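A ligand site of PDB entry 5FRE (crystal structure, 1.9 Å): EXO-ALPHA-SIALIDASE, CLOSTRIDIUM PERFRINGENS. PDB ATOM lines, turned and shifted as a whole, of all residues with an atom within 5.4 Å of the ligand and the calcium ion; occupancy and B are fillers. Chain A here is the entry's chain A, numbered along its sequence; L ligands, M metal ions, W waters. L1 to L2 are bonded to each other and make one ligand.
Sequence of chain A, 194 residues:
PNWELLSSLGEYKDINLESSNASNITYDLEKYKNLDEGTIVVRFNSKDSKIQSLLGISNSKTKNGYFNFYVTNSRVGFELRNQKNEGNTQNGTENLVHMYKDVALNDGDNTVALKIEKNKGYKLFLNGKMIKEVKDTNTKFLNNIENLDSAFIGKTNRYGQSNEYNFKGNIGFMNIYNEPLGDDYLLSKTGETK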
ATOM      1  N   ILE A  51       6.529 -15.541  11.164  1.00  0.00           N
ATOM      2  CA  ILE A  51       6.051 -16.294   9.988  1.00  0.00           C
ATOM      3  C   ILE A  51       5.139 -15.338   9.230  1.00  0.00           C
ATOM      4  O   ILE A  51       4.213 -14.780   9.825  1.00  0.00           O
ATOM      5  CB  ILE A  51       5.265 -17.568  10.393  1.00  0.00           C
ATOM      6  CG1 ILE A  51       6.238 -18.653  10.883  1.00  0.00           C
ATOM      7  CG2 ILE A  51       4.468 -18.127   9.232  1.00  0.00           C
ATOM      8  CD1 ILE A  51       5.604 -19.644  11.814  1.00  0.00           C
ATOM      9  N   SER A  60     -11.804 -18.883   4.394  1.00  0.00           N
ATOM     10  CA  SER A  60     -11.859 -17.936   5.494  1.00  0.00           C
ATOM     11  C   SER A  60     -12.925 -18.249   6.562  1.00  0.00           C
ATOM     12  O   SER A  60     -12.886 -17.628   7.625  1.00  0.00           O
ATOM     13  CB  SER A  60     -12.119 -16.529   4.992  1.00  0.00           C
ATOM     14  OG  SER A  60     -13.476 -16.416   4.578  1.00  0.00           O
ATOM     15  N   LYS A  63     -10.650 -21.981  10.610  1.00  0.00           N
ATOM     16  CA  LYS A  63      -9.380 -21.594  11.169  1.00  0.00           C
ATOM     17  C   LYS A  63      -8.246 -22.222  10.391  1.00  0.00           C
ATOM     18  O   LYS A  63      -7.188 -21.611  10.262  1.00  0.00           O
ATOM     19  CB  LYS A  63      -9.278 -22.027  12.629  1.00  0.00           C
ATOM     20  CG  LYS A  63     -10.351 -21.417  13.503  1.00  0.00           C
ATOM     21  CD  LYS A  63     -10.047 -21.681  14.972  1.00  0.00           C
ATOM     22  CE  LYS A  63     -10.808 -20.686  15.830  1.00  0.00           C
ATOM     23  NZ  LYS A  63     -10.348 -20.745  17.246  1.00  0.00           N
ATOM     24  N   ASN A  64      -8.438 -23.444   9.875  1.00  0.00           N
ATOM     25  CA  ASN A  64      -7.293 -24.213   9.373  1.00  0.00           C
ATOM     26  C   ASN A  64      -7.453 -24.769   7.936  1.00  0.00           C
ATOM     27  O   ASN A  64      -6.733 -25.683   7.580  1.00  0.00           O
ATOM     28  CB  ASN A  64      -6.931 -25.379  10.304  1.00  0.00           C
ATOM     29  CG  ASN A  64      -6.688 -24.952  11.729  1.00  0.00           C
ATOM     30  OD1 ASN A  64      -6.031 -23.951  11.987  1.00  0.00           O
ATOM     31  ND2 ASN A  64      -7.228 -25.757  12.697  1.00  0.00           N
ATOM     32  N   TYR A  66      -6.418 -23.845   4.650  1.00  0.00           N
ATOM     33  CA  TYR A  66      -5.581 -22.918   3.899  1.00  0.00           C
ATOM     34  C   TYR A  66      -4.256 -23.478   3.359  1.00  0.00           C
ATOM     35  O   TYR A  66      -3.757 -24.536   3.784  1.00  0.00           O
ATOM     36  CB  TYR A  66      -5.276 -21.696   4.755  1.00  0.00           C
ATOM     37  CG  TYR A  66      -4.378 -21.931   5.942  1.00  0.00           C
ATOM     38  CD1 TYR A  66      -2.998 -21.954   5.793  1.00  0.00           C
ATOM     39  CD2 TYR A  66      -4.897 -22.098   7.255  1.00  0.00           C
ATOM     40  CE1 TYR A  66      -2.163 -22.151   6.880  1.00  0.00           C
ATOM     41  CE2 TYR A  66      -4.051 -22.272   8.347  1.00  0.00           C
ATOM     42  CZ  TYR A  66      -2.691 -22.296   8.150  1.00  0.00           C
ATOM     43  OH  TYR A  66      -1.801 -22.464   9.210  1.00  0.00           O
ATOM     44  N   ASN A  68      -0.494 -21.710   2.689  1.00  0.00           N
ATOM     45  CA  ASN A  68       0.295 -20.576   3.164  1.00  0.00           C
ATOM     46  C   ASN A  68       1.713 -20.804   2.726  1.00  0.00           C
ATOM     47  O   ASN A  68       2.366 -21.706   3.223  1.00  0.00           O
ATOM     48  CB  ASN A  68       0.134 -20.491   4.709  1.00  0.00           C
ATOM     49  CG  ASN A  68       1.188 -19.619   5.380  1.00  0.00           C
ATOM     50  OD1 ASN A  68       1.637 -18.650   4.834  1.00  0.00           O
ATOM     51  ND2 ASN A  68       1.585 -20.006   6.595  1.00  0.00           N
ATOM     52  N   TYR A  70       5.077 -19.239   2.864  1.00  0.00           N
ATOM     53  CA  TYR A  70       5.575 -18.301   3.874  1.00  0.00           C
ATOM     54  C   TYR A  70       7.078 -18.205   3.988  1.00  0.00           C
ATOM     55  O   TYR A  70       7.831 -19.071   3.553  1.00  0.00           O
ATOM     56  CB  TYR A  70       5.055 -18.608   5.258  1.00  0.00           C
ATOM     57  CG  TYR A  70       5.656 -19.832   5.904  1.00  0.00           C
ATOM     58  CD1 TYR A  70       6.845 -19.768   6.618  1.00  0.00           C
ATOM     59  CD2 TYR A  70       5.044 -21.092   5.772  1.00  0.00           C
ATOM     60  CE1 TYR A  70       7.410 -20.894   7.199  1.00  0.00           C
ATOM     61  CE2 TYR A  70       5.593 -22.247   6.372  1.00  0.00           C
ATOM     62  CZ  TYR A  70       6.789 -22.143   7.077  1.00  0.00           C
ATOM     63  OH  TYR A  70       7.343 -23.251   7.708  1.00  0.00           O
ATOM     64  N   GLU A  79       2.657 -24.516   4.012  1.00  0.00           N
ATOM     65  CA  GLU A  79       1.738 -25.446   4.614  1.00  0.00           C
ATOM     66  C   GLU A  79       0.493 -25.526   3.780  1.00  0.00           C
ATOM     67  O   GLU A  79       0.071 -24.549   3.221  1.00  0.00           O
ATOM     68  CB  GLU A  79       1.303 -25.060   6.018  1.00  0.00           C
ATOM     69  CG  GLU A  79       1.926 -23.872   6.734  1.00  0.00           C
ATOM     70  CD  GLU A  79       1.149 -23.534   8.008  1.00  0.00           C
ATOM     71  OE1 GLU A  79       0.790 -24.492   8.742  1.00  0.00           O
ATOM     72  OE2 GLU A  79       0.935 -22.324   8.286  1.00  0.00           O
ATOM     73  N   ARG A  81      -3.327 -27.180   4.480  1.00  0.00           N
ATOM     74  CA  ARG A  81      -4.202 -27.755   5.490  1.00  0.00           C
ATOM     75  C   ARG A  81      -5.652 -27.617   5.027  1.00  0.00           C
ATOM     76  O   ARG A  81      -6.011 -26.693   4.321  1.00  0.00           O
ATOM     77  CB  ARG A  81      -4.060 -27.016   6.820  1.00  0.00           C
ATOM     78  CG  ARG A  81      -2.642 -26.864   7.324  1.00  0.00           C
ATOM     79  CD  ARG A  81      -2.560 -25.925   8.491  1.00  0.00           C
ATOM     80  NE  ARG A  81      -3.011 -26.531   9.724  1.00  0.00           N
ATOM     81  CZ  ARG A  81      -3.211 -25.881  10.871  1.00  0.00           C
ATOM     82  NH1 ARG A  81      -3.010 -24.558  11.000  1.00  0.00           N
ATOM     83  NH2 ARG A  81      -3.677 -26.574  11.916  1.00  0.00           N
ATOM     84  N   GLN A  90     -11.358 -26.448  16.417  1.00  0.00           N
ATOM     85  CA  GLN A  90     -10.237 -27.168  15.805  1.00  0.00           C
ATOM     86  C   GLN A  90     -10.737 -28.418  15.087  1.00  0.00           C
ATOM     87  O   GLN A  90      -9.968 -29.083  14.411  1.00  0.00           O
ATOM     88  CB  GLN A  90      -9.181 -27.583  16.840  1.00  0.00           C
ATOM     89  CG  GLN A  90      -8.441 -26.423  17.476  1.00  0.00           C
ATOM     90  CD  GLN A  90      -7.624 -25.640  16.456  1.00  0.00           C
ATOM     91  OE1 GLN A  90      -6.958 -26.224  15.597  1.00  0.00           O
ATOM     92  NE2 GLN A  90      -7.729 -24.315  16.491  1.00  0.00           N
ATOM     93  N   HIS A  98       3.447 -30.027   5.328  1.00  0.00           N
ATOM     94  CA  HIS A  98       4.259 -28.920   5.762  1.00  0.00           C
ATOM     95  C   HIS A  98       5.687 -29.157   5.272  1.00  0.00           C
ATOM     96  O   HIS A  98       6.322 -30.148   5.625  1.00  0.00           O
ATOM     97  CB  HIS A  98       4.235 -28.747   7.292  1.00  0.00           C
ATOM     98  CG  HIS A  98       4.906 -27.481   7.754  1.00  0.00           C
ATOM     99  ND1 HIS A  98       5.244 -27.262   9.066  1.00  0.00           N
ATOM    100  CD2 HIS A  98       5.375 -26.414   7.070  1.00  0.00           C
ATOM    101  CE1 HIS A  98       5.854 -26.088   9.174  1.00  0.00           C
ATOM    102  NE2 HIS A  98       5.934 -25.544   7.967  1.00  0.00           N
ATOM    103  N   ASN A 157      -6.110 -15.277   5.033  1.00  0.00           N
ATOM    104  CA  ASN A 157      -7.407 -14.940   5.622  1.00  0.00           C
ATOM    105  C   ASN A 157      -8.069 -16.125   6.296  1.00  0.00           C
ATOM    106  O   ASN A 157      -8.524 -17.064   5.642  1.00  0.00           O
ATOM    107  CB  ASN A 157      -8.318 -14.269   4.537  1.00  0.00           C
ATOM    108  CG  ASN A 157      -9.666 -13.830   5.096  1.00  0.00           C
ATOM    109  OD1 ASN A 157      -9.789 -13.653   6.301  1.00  0.00           O
ATOM    110  ND2 ASN A 157     -10.685 -13.703   4.246  1.00  0.00           N
ATOM    111  N   ARG A 158      -8.110 -16.103   7.621  1.00  0.00           N
ATOM    112  CA  ARG A 158      -8.585 -17.232   8.413  1.00  0.00           C
ATOM    113  C   ARG A 158      -9.762 -16.832   9.298  1.00  0.00           C
ATOM    114  O   ARG A 158     -10.006 -15.663   9.527  1.00  0.00           O
ATOM    115  CB  ARG A 158      -7.424 -17.718   9.306  1.00  0.00           C
ATOM    116  CG  ARG A 158      -6.200 -18.153   8.543  1.00  0.00           C
ATOM    117  CD  ARG A 158      -5.017 -18.499   9.466  1.00  0.00           C
ATOM    118  NE  ARG A 158      -5.255 -19.703  10.256  1.00  0.00           N
ATOM    119  CZ  ARG A 158      -4.406 -20.208  11.164  1.00  0.00           C
ATOM    120  NH1 ARG A 158      -3.241 -19.613  11.401  1.00  0.00           N
ATOM    121  NH2 ARG A 158      -4.707 -21.321  11.813  1.00  0.00           N
ATOM    122  N   TYR A 159     -10.465 -17.796   9.853  1.00  0.00           N
ATOM    123  CA  TYR A 159     -11.617 -17.515  10.694  1.00  0.00           C
ATOM    124  C   TYR A 159     -11.181 -16.852  12.001  1.00  0.00           C
ATOM    125  O   TYR A 159     -10.175 -17.208  12.608  1.00  0.00           O
ATOM    126  CB  TYR A 159     -12.465 -18.760  11.003  1.00  0.00           C
ATOM    127  CG  TYR A 159     -13.633 -18.425  11.920  1.00  0.00           C
ATOM    128  CD1 TYR A 159     -14.830 -17.943  11.399  1.00  0.00           C
ATOM    129  CD2 TYR A 159     -13.506 -18.513  13.305  1.00  0.00           C
ATOM    130  CE1 TYR A 159     -15.884 -17.617  12.222  1.00  0.00           C
ATOM    131  CE2 TYR A 159     -14.549 -18.153  14.140  1.00  0.00           C
ATOM    132  CZ  TYR A 159     -15.728 -17.726  13.596  1.00  0.00           C
ATOM    133  OH  TYR A 159     -16.752 -17.377  14.419  1.00  0.00           O
ATOM    134  N   GLY A 160     -11.985 -15.862  12.411  1.00  0.00           N
ATOM    135  CA  GLY A 160     -11.828 -15.201  13.702  1.00  0.00           C
ATOM    136  C   GLY A 160     -10.465 -14.664  14.046  1.00  0.00           C
ATOM    137  O   GLY A 160      -9.876 -13.895  13.304  1.00  0.00           O
ATOM    138  N   ASN A 163      -4.020 -16.499  13.561  1.00  0.00           N
ATOM    139  CA  ASN A 163      -2.855 -15.794  13.080  1.00  0.00           C
ATOM    140  C   ASN A 163      -2.860 -15.705  11.545  1.00  0.00           C
ATOM    141  O   ASN A 163      -2.837 -16.739  10.865  1.00  0.00           O
ATOM    142  CB  ASN A 163      -1.606 -16.502  13.573  1.00  0.00           C
ATOM    143  CG  ASN A 163      -0.328 -15.781  13.191  1.00  0.00           C
ATOM    144  OD1 ASN A 163      -0.374 -14.735  12.583  1.00  0.00           O
ATOM    145  ND2 ASN A 163       0.821 -16.343  13.571  1.00  0.00           N
ATOM    146  N   GLU A 164      -2.939 -14.486  11.003  1.00  0.00           N
ATOM    147  CA  GLU A 164      -3.007 -14.310   9.525  1.00  0.00           C
ATOM    148  C   GLU A 164      -1.647 -14.155   8.865  1.00  0.00           C
ATOM    149  O   GLU A 164      -1.575 -13.904   7.677  1.00  0.00           O
ATOM    150  CB  GLU A 164      -3.870 -13.086   9.192  1.00  0.00           C
ATOM    151  CG  GLU A 164      -5.314 -13.317   9.583  1.00  0.00           C
ATOM    152  CD  GLU A 164      -6.240 -12.202   9.129  1.00  0.00           C
ATOM    153  OE1 GLU A 164      -5.783 -11.025   9.090  1.00  0.00           O
ATOM    154  OE2 GLU A 164      -7.421 -12.571   8.849  1.00  0.00           O
ATOM    155  N   TYR A 165      -0.581 -14.260   9.649  1.00  0.00           N
ATOM    156  CA  TYR A 165       0.775 -14.250   9.144  1.00  0.00           C
ATOM    157  C   TYR A 165       1.027 -13.029   8.275  1.00  0.00           C
ATOM    158  O   TYR A 165       1.516 -13.129   7.125  1.00  0.00           O
ATOM    159  CB  TYR A 165       1.043 -15.527   8.328  1.00  0.00           C
ATOM    160  CG  TYR A 165       0.652 -16.854   8.956  1.00  0.00           C
ATOM    161  CD1 TYR A 165       1.234 -17.300  10.165  1.00  0.00           C
ATOM    162  CD2 TYR A 165      -0.286 -17.675   8.354  1.00  0.00           C
ATOM    163  CE1 TYR A 165       0.892 -18.510  10.749  1.00  0.00           C
ATOM    164  CE2 TYR A 165      -0.632 -18.919   8.914  1.00  0.00           C
ATOM    165  CZ  TYR A 165      -0.034 -19.338  10.105  1.00  0.00           C
ATOM    166  OH  TYR A 165      -0.425 -20.536  10.654  1.00  0.00           O
HETATM  167  C1  LIG L   1      -1.431 -22.439  19.041  1.00  0.00           C
HETATM  168  C2  LIG L   1      -0.886 -23.171  17.820  1.00  0.00           C
HETATM  169  C3  LIG L   1      -1.486 -22.648  16.536  1.00  0.00           C
HETATM  170  C4  LIG L   1      -2.987 -22.378  16.681  1.00  0.00           C
HETATM  171  C5  LIG L   1      -3.451 -21.749  17.979  1.00  0.00           C
HETATM  172  C6  LIG L   1      -4.967 -21.865  18.142  1.00  0.00           C
HETATM  173  O1  LIG L   1      -1.068 -23.252  20.172  1.00  0.00           O
HETATM  174  O2  LIG L   1       0.523 -22.965  17.796  1.00  0.00           O
HETATM  175  O3  LIG L   1      -1.224 -23.642  15.488  1.00  0.00           O
HETATM  176  O4  LIG L   1      -3.678 -23.600  16.568  1.00  0.00           O
HETATM  177  O5  LIG L   1      -2.860 -22.435  19.048  1.00  0.00           O
HETATM  178  O6  LIG L   1      -5.443 -20.796  18.959  1.00  0.00           O
HETATM  179  C1  LG2 L   2      -1.813 -22.024  13.731  1.00  0.00           C
HETATM  180  C2  LG2 L   2      -0.727 -22.924  14.348  1.00  0.00           C
HETATM  181  C3  LG2 L   2      -0.419 -24.175  13.488  1.00  0.00           C
HETATM  182  C4  LG2 L   2       0.297 -23.750  12.176  1.00  0.00           C
HETATM  183  C5  LG2 L   2       1.551 -22.943  12.477  1.00  0.00           C
HETATM  184  C6  LG2 L   2       1.154 -21.747  13.346  1.00  0.00           C
HETATM  185  C7  LG2 L   2       2.339 -20.902  13.716  1.00  0.00           C
HETATM  186  C8  LG2 L   2       1.946 -19.755  14.646  1.00  0.00           C
HETATM  187  C9  LG2 L   2       2.988 -18.687  14.459  1.00  0.00           C
HETATM  188  C10 LG2 L   2       3.471 -22.638  10.946  1.00  0.00           C
HETATM  189  C11 LG2 L   2       3.984 -22.192   9.598  1.00  0.00           C
HETATM  190  N1  LG2 L   2       2.175 -22.493  11.221  1.00  0.00           N
HETATM  191  O1  LG2 L   2      -2.845 -22.572  13.260  1.00  0.00           O
HETATM  192  O2  LG2 L   2      -1.690 -20.763  13.774  1.00  0.00           O
HETATM  193  O3  LG2 L   2       0.657 -24.873  11.383  1.00  0.00           O
HETATM  194  O4  LG2 L   2       0.523 -22.255  14.512  1.00  0.00           O
HETATM  195  O5  LG2 L   2       3.325 -21.712  14.356  1.00  0.00           O
HETATM  196  O6  LG2 L   2       0.636 -19.195  14.423  1.00  0.00           O
HETATM  197  O7  LG2 L   2       2.796 -17.914  15.610  1.00  0.00           O
HETATM  198  O8  LG2 L   2       4.230 -23.069  11.733  1.00  0.00           O
HETATM  199 CA    CA M   1     -10.467 -13.479   8.566  1.00  0.00          CA
HETATM  200  O   HOH W   1      -3.743 -19.185  14.796  1.00  0.00           O
HETATM  201  O   HOH W   2      -9.620 -11.275   8.096  1.00  0.00           O
HETATM  202  O   HOH W   3     -12.352 -14.831   8.097  1.00  0.00           O
HETATM  203  O   HOH W   4       0.154 -17.397  16.789  1.00  0.00           O
HETATM  204  O   HOH W   5     -12.370 -11.844   8.205  1.00  0.00           O
HETATM  205  O   HOH W   6       3.198 -26.471  11.868  1.00  0.00           O
HETATM  206  O   HOH W   7      -3.717 -25.287  14.711  1.00  0.00           O
HETATM  207  O   HOH W   8     -11.027 -13.155  10.881  1.00  0.00           O
HETATM  208  O   HOH W   9      -1.007 -21.453  21.908  1.00  0.00           O
HETATM  209  O   HOH W  10      -5.977 -22.987  14.548  1.00  0.00           O
HETATM  210  O   HOH W  11       6.646 -23.412  12.437  1.00  0.00           O
HETATM  211  O   HOH W  12       2.712 -23.365  16.373  1.00  0.00           O
HETATM  212  O   HOH W  13       4.019 -15.229  15.061  1.00  0.00           O
HETATM  213  O   HOH W  14      -7.802 -19.433  17.101  1.00  0.00           O
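An oxygen (O1) of LG2 L2 is in salt-bridge range of the guanidinium group of Arg 158, at 2.7 Å. OE1 of Glu 79 lies within hydrogen-bond range of O3 of LG2 L2, 2.7 Å away. ND2 of Asn 163 is in hydrogen-bond range of O6 of LG2 L2. NH1 of Arg 81 lies within salt-bridge range of O1 of LG2 L2 (3.0 Å). OH of Tyr 165 lies within hydrogen-bond range of N1 of LG2 L2 (3.3 Å).
The guanidinium group of Arg 158 lies within hydrogen-bond range of the backbone carbonyl oxygen of Asn 163. NH1 of Arg 158 lies within hydrogen-bond range of OH of Tyr 165 (3.1 Å). The side-chain carboxylate (OE2) of Glu 79 lies within hydrogen-bond range of the side-chain hydroxyl (OH) of Tyr 165, at 3.3 Å. OE2 of Glu 79 sits at hydrogen-bond distance from OH of Tyr 66. The backbone NH (N) of Tyr 165 lies within hydrogen-bond range of the side-chain amide oxygen (OD1) of Asn 163 (3.0 Å). The side-chain amide oxygen (OD1) of Asn 64 sits at hydrogen-bond distance from the guanidinium group (NH1) of Arg 81, 3.2 Å away. The backbone carbonyl oxygen (O) of Tyr 66 lies within hydrogen-bond range of the backbone NH (N) of Arg 81 (2.8 Å). OH of Tyr 165 lies within hydrogen-bond range of OH of Tyr 66 (2.8 Å).
Residues that only touch the ligand: Tyr 70 (3.6 Å), Ile 51 (3.7 Å), Asn 64 (3.7 Å) and Tyr 66 (3.9 Å). Hydrophobic or aromatic side chains that line the ligand: Ile 51, Tyr 70 and Tyr 165.
OE2 of Glu 164 touches the calcium ion, at 3.2 Å. Three residues have an atom within 4 Å of the calcium ion: Asn 157, Arg 158 and Glu 164.
The calcium ion is bound by water W3, the side-chain amide oxygen (OD1) of Asn 157, water W8, water W2, the backbone carbonyl oxygen (O) of Arg 158 and water W5.
Water W7 lies within hydrogen-bond range of an oxygen (O4) of LIG L1 (2.5 Å), the guanidinium group (NH2) of Arg 81 (3.1 Å) and the side-chain amide oxygen (OE1) of Gln 90 (3.5 Å). Water W1 lies within hydrogen-bond range of O2 of LG2 L2, N of Asn 163 and NH1 of Arg 158. Water W4 bridges O7 of LG2 L2 (2.9 Å) and ND2 of Asn 163 (3.5 Å). Water W10 lies within hydrogen-bond range of OD1 of Asn 64, NE2 of Gln 90, O4 of LIG L1 and NH2 of Arg 158. Water W14 lies within hydrogen-bond range of NZ of Lys 63 (2.9 Å) and O6 of LIG L1 (3.3 Å).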
